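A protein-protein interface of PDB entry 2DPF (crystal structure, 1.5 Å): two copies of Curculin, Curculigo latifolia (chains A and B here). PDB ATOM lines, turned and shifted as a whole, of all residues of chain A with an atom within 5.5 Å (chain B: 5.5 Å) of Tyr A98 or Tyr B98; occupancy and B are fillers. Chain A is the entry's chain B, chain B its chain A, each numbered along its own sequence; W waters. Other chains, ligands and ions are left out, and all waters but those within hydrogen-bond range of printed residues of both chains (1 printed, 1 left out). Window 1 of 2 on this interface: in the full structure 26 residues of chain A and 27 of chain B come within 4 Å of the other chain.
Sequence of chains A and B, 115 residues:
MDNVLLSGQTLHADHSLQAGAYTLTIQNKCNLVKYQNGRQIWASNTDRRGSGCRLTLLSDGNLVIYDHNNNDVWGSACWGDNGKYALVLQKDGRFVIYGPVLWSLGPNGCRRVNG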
ATOM      1  N   LEU A   6      23.043 -13.438  15.499  1.00  0.00           N
ATOM      2  CA  LEU A   6      23.228 -14.869  15.732  1.00  0.00           C
ATOM      3  C   LEU A   6      22.310 -15.358  16.834  1.00  0.00           C
ATOM      4  O   LEU A   6      21.845 -14.564  17.647  1.00  0.00           O
ATOM      5  CB  LEU A   6      24.664 -15.156  16.160  1.00  0.00           C
ATOM      6  CG  LEU A   6      25.791 -14.787  15.196  1.00  0.00           C
ATOM      7  CD1 LEU A   6      27.134 -15.130  15.825  1.00  0.00           C
ATOM      8  CD2 LEU A   6      25.590 -15.536  13.884  1.00  0.00           C
ATOM      9  N   LYS A  84      22.347 -23.713  16.253  1.00  0.00           N
ATOM     10  CA  LYS A  84      22.812 -22.350  16.072  1.00  0.00           C
ATOM     11  C   LYS A  84      22.348 -21.857  14.705  1.00  0.00           C
ATOM     12  O   LYS A  84      22.516 -22.549  13.695  1.00  0.00           O
ATOM     13  CB  LYS A  84      24.335 -22.331  16.145  1.00  0.00           C
ATOM     14  CG  LYS A  84      24.951 -20.998  16.490  1.00  0.00           C
ATOM     15  CD  LYS A  84      25.052 -20.807  17.990  1.00  0.00           C
ATOM     16  CE  LYS A  84      25.829 -19.536  18.340  1.00  0.00           C
ATOM     17  NZ  LYS A  84      25.016 -18.292  18.257  1.00  0.00           N
ATOM     18  N   TYR A  85      21.770 -20.662  14.689  1.00  0.00           N
ATOM     19  CA  TYR A  85      21.269 -20.051  13.466  1.00  0.00           C
ATOM     20  C   TYR A  85      21.809 -18.644  13.295  1.00  0.00           C
ATOM     21  O   TYR A  85      22.371 -18.050  14.221  1.00  0.00           O
ATOM     22  CB  TYR A  85      19.740 -19.992  13.488  1.00  0.00           C
ATOM     23  CG  TYR A  85      19.090 -21.352  13.498  1.00  0.00           C
ATOM     24  CD1 TYR A  85      18.478 -21.867  12.347  1.00  0.00           C
ATOM     25  CD2 TYR A  85      19.125 -22.154  14.645  1.00  0.00           C
ATOM     26  CE1 TYR A  85      17.927 -23.142  12.337  1.00  0.00           C
ATOM     27  CE2 TYR A  85      18.572 -23.439  14.646  1.00  0.00           C
ATOM     28  CZ  TYR A  85      17.979 -23.925  13.487  1.00  0.00           C
ATOM     29  OH  TYR A  85      17.470 -25.207  13.458  1.00  0.00           O
ATOM     30  N   ALA A  86      21.617 -18.096  12.102  1.00  0.00           N
ATOM     31  CA  ALA A  86      22.080 -16.752  11.826  1.00  0.00           C
ATOM     32  C   ALA A  86      21.058 -15.982  11.015  1.00  0.00           C
ATOM     33  O   ALA A  86      20.616 -16.456   9.964  1.00  0.00           O
ATOM     34  CB  ALA A  86      23.406 -16.803  11.054  1.00  0.00           C
ATOM     35  N   LEU A  87      20.668 -14.808  11.511  1.00  0.00           N
ATOM     36  CA  LEU A  87      19.742 -13.949  10.787  1.00  0.00           C
ATOM     37  C   LEU A  87      20.621 -12.953  10.048  1.00  0.00           C
ATOM     38  O   LEU A  87      21.433 -12.249  10.655  1.00  0.00           O
ATOM     39  CB  LEU A  87      18.812 -13.181  11.735  1.00  0.00           C
ATOM     40  CG  LEU A  87      17.991 -12.063  11.073  1.00  0.00           C
ATOM     41  CD1 LEU A  87      16.969 -12.663  10.118  1.00  0.00           C
ATOM     42  CD2 LEU A  87      17.274 -11.234  12.147  1.00  0.00           C
ATOM     43  N   VAL A  88      20.455 -12.893   8.734  1.00  0.00           N
ATOM     44  CA  VAL A  88      21.243 -11.985   7.923  1.00  0.00           C
ATOM     45  C   VAL A  88      20.365 -10.993   7.173  1.00  0.00           C
ATOM     46  O   VAL A  88      19.438 -11.395   6.468  1.00  0.00           O
ATOM     47  CB  VAL A  88      22.073 -12.757   6.855  1.00  0.00           C
ATOM     48  CG1 VAL A  88      22.957 -11.787   6.080  1.00  0.00           C
ATOM     49  CG2 VAL A  88      22.919 -13.841   7.513  1.00  0.00           C
ATOM     50  N   GLN A  90      20.364  -8.976   4.250  1.00  0.00           N
ATOM     51  CA  GLN A  90      21.128  -8.983   3.007  1.00  0.00           C
ATOM     52  C   GLN A  90      21.112  -7.657   2.262  1.00  0.00           C
ATOM     53  O   GLN A  90      20.228  -6.819   2.474  1.00  0.00           O
ATOM     54  CB  GLN A  90      20.609 -10.119   2.127  1.00  0.00           C
ATOM     55  CG  GLN A  90      21.031 -11.481   2.671  1.00  0.00           C
ATOM     56  CD  GLN A  90      20.315 -12.665   2.051  1.00  0.00           C
ATOM     57  OE1 GLN A  90      19.651 -12.561   1.017  1.00  0.00           O
ATOM     58  NE2 GLN A  90      20.462 -13.817   2.689  1.00  0.00           N
ATOM     59  N   VAL A  96      17.055 -12.958   6.107  1.00  0.00           N
ATOM     60  CA  VAL A  96      16.897 -14.397   6.071  1.00  0.00           C
ATOM     61  C   VAL A  96      17.543 -15.094   7.257  1.00  0.00           C
ATOM     62  O   VAL A  96      18.622 -14.705   7.719  1.00  0.00           O
ATOM     63  CB  VAL A  96      17.552 -14.942   4.764  1.00  0.00           C
ATOM     64  CG1 VAL A  96      17.365 -16.457   4.644  1.00  0.00           C
ATOM     65  CG2 VAL A  96      16.982 -14.203   3.561  1.00  0.00           C
ATOM     66  N   ILE A  97      16.868 -16.121   7.755  1.00  0.00           N
ATOM     67  CA  ILE A  97      17.426 -16.903   8.851  1.00  0.00           C
ATOM     68  C   ILE A  97      17.978 -18.187   8.254  1.00  0.00           C
ATOM     69  O   ILE A  97      17.249 -18.952   7.631  1.00  0.00           O
ATOM     70  CB  ILE A  97      16.369 -17.240   9.916  1.00  0.00           C
ATOM     71  CG1 ILE A  97      15.824 -15.950  10.511  1.00  0.00           C
ATOM     72  CG2 ILE A  97      16.983 -18.087  11.021  1.00  0.00           C
ATOM     73  CD1 ILE A  97      14.738 -16.158  11.556  1.00  0.00           C
ATOM     74  N   TYR A  98      19.284 -18.389   8.425  1.00  0.00           N
ATOM     75  CA  TYR A  98      19.990 -19.567   7.930  1.00  0.00           C
ATOM     76  C   TYR A  98      20.382 -20.460   9.097  1.00  0.00           C
ATOM     77  O   TYR A  98      20.830 -19.969  10.138  1.00  0.00           O
ATOM     78  CB  TYR A  98      21.285 -19.151   7.238  1.00  0.00           C
ATOM     79  CG  TYR A  98      21.108 -18.380   5.962  1.00  0.00           C
ATOM     80  CD1 TYR A  98      20.973 -19.044   4.736  1.00  0.00           C
ATOM     81  CD2 TYR A  98      21.098 -16.988   5.970  1.00  0.00           C
ATOM     82  CE1 TYR A  98      20.840 -18.334   3.558  1.00  0.00           C
ATOM     83  CE2 TYR A  98      20.960 -16.268   4.797  1.00  0.00           C
ATOM     84  CZ  TYR A  98      20.832 -16.952   3.593  1.00  0.00           C
ATOM     85  OH  TYR A  98      20.679 -16.255   2.420  1.00  0.00           O
ATOM     86  N   GLY A  99      20.214 -21.762   8.924  1.00  0.00           N
ATOM     87  CA  GLY A  99      20.608 -22.684   9.967  1.00  0.00           C
ATOM     88  C   GLY A  99      19.983 -24.057   9.866  1.00  0.00           C
ATOM     89  O   GLY A  99      19.112 -24.284   9.032  1.00  0.00           O
ATOM     90  N   PRO A 100      20.408 -24.994  10.726  1.00  0.00           N
ATOM     91  CA  PRO A 100      21.434 -24.771  11.750  1.00  0.00           C
ATOM     92  C   PRO A 100      22.852 -24.771  11.165  1.00  0.00           C
ATOM     93  O   PRO A 100      23.041 -24.669   9.947  1.00  0.00           O
ATOM     94  CB  PRO A 100      21.193 -25.921  12.721  1.00  0.00           C
ATOM     95  CG  PRO A 100      20.790 -27.024  11.810  1.00  0.00           C
ATOM     96  CD  PRO A 100      19.810 -26.331  10.873  1.00  0.00           C
ATOM     97  N   VAL A 101      23.850 -24.875  12.032  1.00  0.00           N
ATOM     98  CA  VAL A 101      25.226 -24.888  11.559  1.00  0.00           C
ATOM     99  C   VAL A 101      25.486 -26.105  10.689  1.00  0.00           C
ATOM    100  O   VAL A 101      25.075 -27.227  11.010  1.00  0.00           O
ATOM    101  CB  VAL A 101      26.234 -24.902  12.738  1.00  0.00           C
ATOM    102  CG1 VAL A 101      27.661 -25.119  12.202  1.00  0.00           C
ATOM    103  CG2 VAL A 101      26.166 -23.593  13.494  1.00  0.00           C
ATOM    104  N   LEU A 102      26.154 -25.872   9.564  1.00  0.00           N
ATOM    105  CA  LEU A 102      26.520 -26.949   8.669  1.00  0.00           C
ATOM    106  C   LEU A 102      27.975 -27.312   8.932  1.00  0.00           C
ATOM    107  O   LEU A 102      28.313 -28.490   9.063  1.00  0.00           O
ATOM    108  CB  LEU A 102      26.400 -26.519   7.201  1.00  0.00           C
ATOM    109  CG  LEU A 102      27.041 -27.482   6.186  1.00  0.00           C
ATOM    110  CD1 LEU A 102      26.368 -28.837   6.251  1.00  0.00           C
ATOM    111  CD2 LEU A 102      26.911 -26.904   4.783  1.00  0.00           C
ATOM    112  N   LEU B   6      27.591 -15.240   0.980  1.00  0.00           N
ATOM    113  CA  LEU B   6      26.413 -16.063   0.726  1.00  0.00           C
ATOM    114  C   LEU B   6      26.750 -17.085  -0.337  1.00  0.00           C
ATOM    115  O   LEU B   6      27.666 -16.870  -1.129  1.00  0.00           O
ATOM    116  CB  LEU B   6      25.249 -15.203   0.236  1.00  0.00           C
ATOM    117  CG  LEU B   6      24.737 -14.136   1.201  1.00  0.00           C
ATOM    118  CD1 LEU B   6      23.541 -13.450   0.565  1.00  0.00           C
ATOM    119  CD2 LEU B   6      24.346 -14.767   2.528  1.00  0.00           C
ATOM    120  N   LYS B  84      20.303 -22.471  -0.053  1.00  0.00           N
ATOM    121  CA  LYS B  84      21.047 -21.241   0.161  1.00  0.00           C
ATOM    122  C   LYS B  84      21.677 -21.281   1.546  1.00  0.00           C
ATOM    123  O   LYS B  84      21.022 -21.617   2.533  1.00  0.00           O
ATOM    124  CB  LYS B  84      20.133 -20.019   0.047  1.00  0.00           C
ATOM    125  CG  LYS B  84      19.768 -19.633  -1.388  1.00  0.00           C
ATOM    126  CD  LYS B  84      18.801 -18.454  -1.392  1.00  0.00           C
ATOM    127  CE  LYS B  84      18.768 -17.742  -2.736  1.00  0.00           C
ATOM    128  NZ  LYS B  84      18.432 -18.666  -3.850  1.00  0.00           N
ATOM    129  N   TYR B  85      22.959 -20.954   1.595  1.00  0.00           N
ATOM    130  CA  TYR B  85      23.727 -20.954   2.830  1.00  0.00           C
ATOM    131  C   TYR B  85      24.438 -19.629   3.050  1.00  0.00           C
ATOM    132  O   TYR B  85      24.537 -18.788   2.151  1.00  0.00           O
ATOM    133  CB  TYR B  85      24.774 -22.074   2.796  1.00  0.00           C
ATOM    134  CG  TYR B  85      24.204 -23.466   2.803  1.00  0.00           C
ATOM    135  CD1 TYR B  85      23.589 -24.008   1.670  1.00  0.00           C
ATOM    136  CD2 TYR B  85      24.237 -24.237   3.963  1.00  0.00           C
ATOM    137  CE1 TYR B  85      23.014 -25.278   1.706  1.00  0.00           C
ATOM    138  CE2 TYR B  85      23.676 -25.500   4.007  1.00  0.00           C
ATOM    139  CZ  TYR B  85      23.065 -26.014   2.882  1.00  0.00           C
ATOM    140  OH  TYR B  85      22.499 -27.261   2.951  1.00  0.00           O
ATOM    141  N   ALA B  86      24.955 -19.450   4.263  1.00  0.00           N
ATOM    142  CA  ALA B  86      25.674 -18.237   4.583  1.00  0.00           C
ATOM    143  C   ALA B  86      26.901 -18.518   5.451  1.00  0.00           C
ATOM    144  O   ALA B  86      26.808 -19.194   6.479  1.00  0.00           O
ATOM    145  CB  ALA B  86      24.743 -17.241   5.298  1.00  0.00           C
ATOM    146  N   LEU B  87      28.055 -18.041   4.988  1.00  0.00           N
ATOM    147  CA  LEU B  87      29.300 -18.163   5.735  1.00  0.00           C
ATOM    148  C   LEU B  87      29.443 -16.841   6.482  1.00  0.00           C
ATOM    149  O   LEU B  87      29.448 -15.772   5.882  1.00  0.00           O
ATOM    150  CB  LEU B  87      30.497 -18.370   4.791  1.00  0.00           C
ATOM    151  CG  LEU B  87      31.891 -18.147   5.392  1.00  0.00           C
ATOM    152  CD1 LEU B  87      32.123 -19.095   6.552  1.00  0.00           C
ATOM    153  CD2 LEU B  87      32.948 -18.377   4.321  1.00  0.00           C
ATOM    154  N   VAL B  88      29.522 -16.923   7.805  1.00  0.00           N
ATOM    155  CA  VAL B  88      29.662 -15.734   8.633  1.00  0.00           C
ATOM    156  C   VAL B  88      30.977 -15.733   9.397  1.00  0.00           C
ATOM    157  O   VAL B  88      31.292 -16.706  10.083  1.00  0.00           O
ATOM    158  CB  VAL B  88      28.512 -15.649   9.680  1.00  0.00           C
ATOM    159  CG1 VAL B  88      28.644 -14.363  10.508  1.00  0.00           C
ATOM    160  CG2 VAL B  88      27.155 -15.694   8.978  1.00  0.00           C
ATOM    161  N   GLN B  90      32.516 -14.446  12.386  1.00  0.00           N
ATOM    162  CA  GLN B  90      32.010 -13.882  13.629  1.00  0.00           C
ATOM    163  C   GLN B  90      33.046 -13.124  14.441  1.00  0.00           C
ATOM    164  O   GLN B  90      34.252 -13.373  14.337  1.00  0.00           O
ATOM    165  CB  GLN B  90      31.384 -15.009  14.434  1.00  0.00           C
ATOM    166  CG  GLN B  90      30.259 -15.652  13.636  1.00  0.00           C
ATOM    167  CD  GLN B  90      29.687 -16.903  14.251  1.00  0.00           C
ATOM    168  OE1 GLN B  90      28.756 -17.492  13.696  1.00  0.00           O
ATOM    169  NE2 GLN B  90      30.230 -17.325  15.389  1.00  0.00           N
ATOM    170  N   VAL B  96      31.640 -19.560  10.466  1.00  0.00           N
ATOM    171  CA  VAL B  96      30.677 -20.642  10.451  1.00  0.00           C
ATOM    172  C   VAL B  96      29.743 -20.607   9.251  1.00  0.00           C
ATOM    173  O   VAL B  96      29.290 -19.541   8.842  1.00  0.00           O
ATOM    174  CB  VAL B  96      29.816 -20.559  11.747  1.00  0.00           C
ATOM    175  CG1 VAL B  96      28.883 -21.739  11.856  1.00  0.00           C
ATOM    176  CG2 VAL B  96      30.737 -20.479  12.959  1.00  0.00           C
ATOM    177  N   ILE B  97      29.462 -21.780   8.705  1.00  0.00           N
ATOM    178  CA  ILE B  97      28.549 -21.890   7.576  1.00  0.00           C
ATOM    179  C   ILE B  97      27.203 -22.349   8.119  1.00  0.00           C
ATOM    180  O   ILE B  97      27.096 -23.427   8.712  1.00  0.00           O
ATOM    181  CB  ILE B  97      29.051 -22.907   6.528  1.00  0.00           C
ATOM    182  CG1 ILE B  97      30.417 -22.458   6.005  1.00  0.00           C
ATOM    183  CG2 ILE B  97      28.031 -23.028   5.381  1.00  0.00           C
ATOM    184  CD1 ILE B  97      31.060 -23.430   5.027  1.00  0.00           C
ATOM    185  N   TYR B  98      26.192 -21.502   7.928  1.00  0.00           N
ATOM    186  CA  TYR B  98      24.827 -21.771   8.374  1.00  0.00           C
ATOM    187  C   TYR B  98      23.910 -22.042   7.189  1.00  0.00           C
ATOM    188  O   TYR B  98      23.977 -21.348   6.172  1.00  0.00           O
ATOM    189  CB  TYR B  98      24.265 -20.556   9.099  1.00  0.00           C
ATOM    190  CG  TYR B  98      24.958 -20.186  10.381  1.00  0.00           C
ATOM    191  CD1 TYR B  98      24.547 -20.732  11.592  1.00  0.00           C
ATOM    192  CD2 TYR B  98      26.017 -19.277  10.389  1.00  0.00           C
ATOM    193  CE1 TYR B  98      25.167 -20.379  12.779  1.00  0.00           C
ATOM    194  CE2 TYR B  98      26.649 -18.917  11.577  1.00  0.00           C
ATOM    195  CZ  TYR B  98      26.212 -19.474  12.770  1.00  0.00           C
ATOM    196  OH  TYR B  98      26.799 -19.114  13.958  1.00  0.00           O
ATOM    197  N   GLY B  99      23.028 -23.020   7.340  1.00  0.00           N
ATOM    198  CA  GLY B  99      22.096 -23.302   6.269  1.00  0.00           C
ATOM    199  C   GLY B  99      21.474 -24.680   6.315  1.00  0.00           C
ATOM    200  O   GLY B  99      21.885 -25.513   7.115  1.00  0.00           O
ATOM    201  N   PRO B 100      20.489 -24.958   5.440  1.00  0.00           N
ATOM    202  CA  PRO B 100      19.980 -24.006   4.445  1.00  0.00           C
ATOM    203  C   PRO B 100      19.028 -22.989   5.072  1.00  0.00           C
ATOM    204  O   PRO B 100      19.018 -22.817   6.287  1.00  0.00           O
ATOM    205  CB  PRO B 100      19.300 -24.914   3.426  1.00  0.00           C
ATOM    206  CG  PRO B 100      18.725 -26.013   4.300  1.00  0.00           C
ATOM    207  CD  PRO B 100      19.839 -26.277   5.306  1.00  0.00           C
ATOM    208  N   VAL B 101      18.233 -22.318   4.244  1.00  0.00           N
ATOM    209  CA  VAL B 101      17.309 -21.315   4.756  1.00  0.00           C
ATOM    210  C   VAL B 101      16.236 -21.954   5.629  1.00  0.00           C
ATOM    211  O   VAL B 101      15.622 -22.955   5.246  1.00  0.00           O
ATOM    212  CB  VAL B 101      16.627 -20.544   3.605  1.00  0.00           C
ATOM    213  CG1 VAL B 101      15.526 -19.646   4.162  1.00  0.00           C
ATOM    214  CG2 VAL B 101      17.652 -19.716   2.851  1.00  0.00           C
ATOM    215  N   LEU B 102      16.032 -21.380   6.811  1.00  0.00           N
ATOM    216  CA  LEU B 102      15.011 -21.866   7.729  1.00  0.00           C
ATOM    217  C   LEU B 102      13.757 -21.040   7.527  1.00  0.00           C
ATOM    218  O   LEU B 102      12.653 -21.579   7.439  1.00  0.00           O
ATOM    219  CB  LEU B 102      15.446 -21.700   9.186  1.00  0.00           C
ATOM    220  CG  LEU B 102      14.322 -21.890  10.225  1.00  0.00           C
ATOM    221  CD1 LEU B 102      13.953 -23.354  10.295  1.00  0.00           C
ATOM    222  CD2 LEU B 102      14.766 -21.416  11.602  1.00  0.00           C
HETATM  223  O   HOH W   1      22.517 -17.459   0.752  1.00  0.00           O
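O of Lys B84 is in hydrogen-bond range of N of Val B101. O of Ala B86 is in hydrogen-bond range of N of Tyr B98 (2.8 Å). OE1 of Gln B90 is in hydrogen-bond range of OH of Tyr B98 (2.6 Å). O of Lys A84 sits at hydrogen-bond distance from N of Val A101, at 3.2 Å. The backbone NH (N) of Val A88 is in hydrogen-bond range of the backbone carbonyl oxygen (O) of Val A96 (2.8 Å). The side-chain amide nitrogen (NE2) of Gln A90 is in hydrogen-bond range of the side-chain hydroxyl (OH) of Tyr A98 (2.5 Å).
The backbone carbonyl oxygen (O) of Ile B97 sits at hydrogen-bond distance from the backbone NH (N) of Leu A102 (2.8 Å). The backbone carbonyl oxygen (O) of Pro A100 lies within hydrogen-bond range of the backbone NH (N) of Gly B99, at 3.1 Å. O of Pro B100 lies within hydrogen-bond range of N of Gly A99, at 3.1 Å. The backbone carbonyl oxygen of Ile A97 sits at hydrogen-bond distance from the backbone NH of Leu B102, at 2.8 Å. The backbone NH of Gly B99 sits close to the backbone NH of Gly A99.
Among the printed residues, merely in contact across the chains: Leu A6 with Gln B90 (3.5 Å), Leu A6 with Tyr B98 (3.8 Å), Lys A84 with Tyr B98 (3.4 Å), Tyr A85 with Tyr B98 (3.8 Å), Tyr A85 with Leu B102 (3.7 Å), Ala A86 with Tyr B98 (3.7 Å), Gln A90 with Leu B6 (3.6 Å), Val A96 with Val B101 (3.7 Å), Ile A97 with Val B101 (3.7 Å), Tyr A98 with Leu B6 (3.96 Å), Tyr A98 with Lys B84 (3.4 Å), Tyr A98 with Tyr B85 (3.9 Å), Tyr A98 with Ala B86 (3.7 Å), Tyr A98 with Tyr B98 (3.6 Å), Tyr A98 with Pro B100 (3.8 Å), Tyr A98 with Val B101 (3.5 Å), Pro A100 with Tyr B98 (3.8 Å), Val A101 with Val B96 (3.6 Å), Val A101 with Ile B97 (3.7 Å), Val A101 with Tyr B98 (3.4 Å) and Leu A102 with Tyr B85 (3.6 Å).
Water W1 lies within hydrogen-bond range of OH of Tyr A98 (2.8 Å) and O of Tyr B85 (2.8 Å).
Of the 14 printed residues of chain B, 12 touch a printed residue of chain A. Printed residues of chain B that touch a printed residue of chain A: Leu B6, Lys B84, Tyr B85, Ala B86, Gln B90, Val B96, Ile B97, Tyr B98, Gly B99, Pro B100, Val B101 and Leu B102. Of the 14 printed residues of chain A, 12 touch a printed residue of chain B. Printed residues of chain A that touch a printed residue of chain B: Leu A6, Lys A84, Tyr A85, Ala A86, Gln A90, Val A96, Ile A97, Tyr A98, Gly A99, Pro A100, Val A101 and Leu A102. Hydrophobic or aromatic side chains of chain A within 4 Å of the printed part of chain B: Leu A6, Tyr A85, Ala A86, Val A96, Tyr A98, Val A101 and Leu A102. Among the printed residues, no Asp or Glu carboxylate lies within 4 Å of a Lys or Arg side-chain nitrogen of the other chain.
Tyr A98 touches just these residues of chain B: Leu B6, Lys B84, Tyr B85, Ala B86, Tyr B98, Pro B100 and Val B101. Tyr B98 touches seven residues of chain A. Printed residues of chain A within 4 Å of Gln B90: Leu A6 (3.5 Å). Printed residues of chain A within 4 Å of Leu B6: Gln A90 and Tyr A98. Of the printed residues of chain A, Ala B86 touches Tyr A98 (3.7 Å). Printed residues of chain A within 4 Å of Lys B84: Tyr A98. Of the printed residues of chain A, Leu B102 touches Tyr A85 and Ile A97. Leu B87 touches none of the printed residues of chain A. The nearest residue of chain A that does not touch Tyr B98 is Gly A99 (4.1 Å).
Ala A86 touches Tyr B98, and with the chains exchanged Tyr A98 touches Ala B86. Val A96 touches Val B101, and with the chains exchanged Val A101 touches Val B96. Ile A97 touches Val B101, and with the chains exchanged Val A101 touches Ile B97. Tyr A98 touches its own counterpart, Tyr B98. Positions printed for both chains: 6, 84, 85, 86, 87, 88, 90, 96, 97, 98, 99, 100, 101 and 102. Of the 26 pairs that touch across the chains among the printed residues, 26 have their exchanged pair printed and touching as well.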
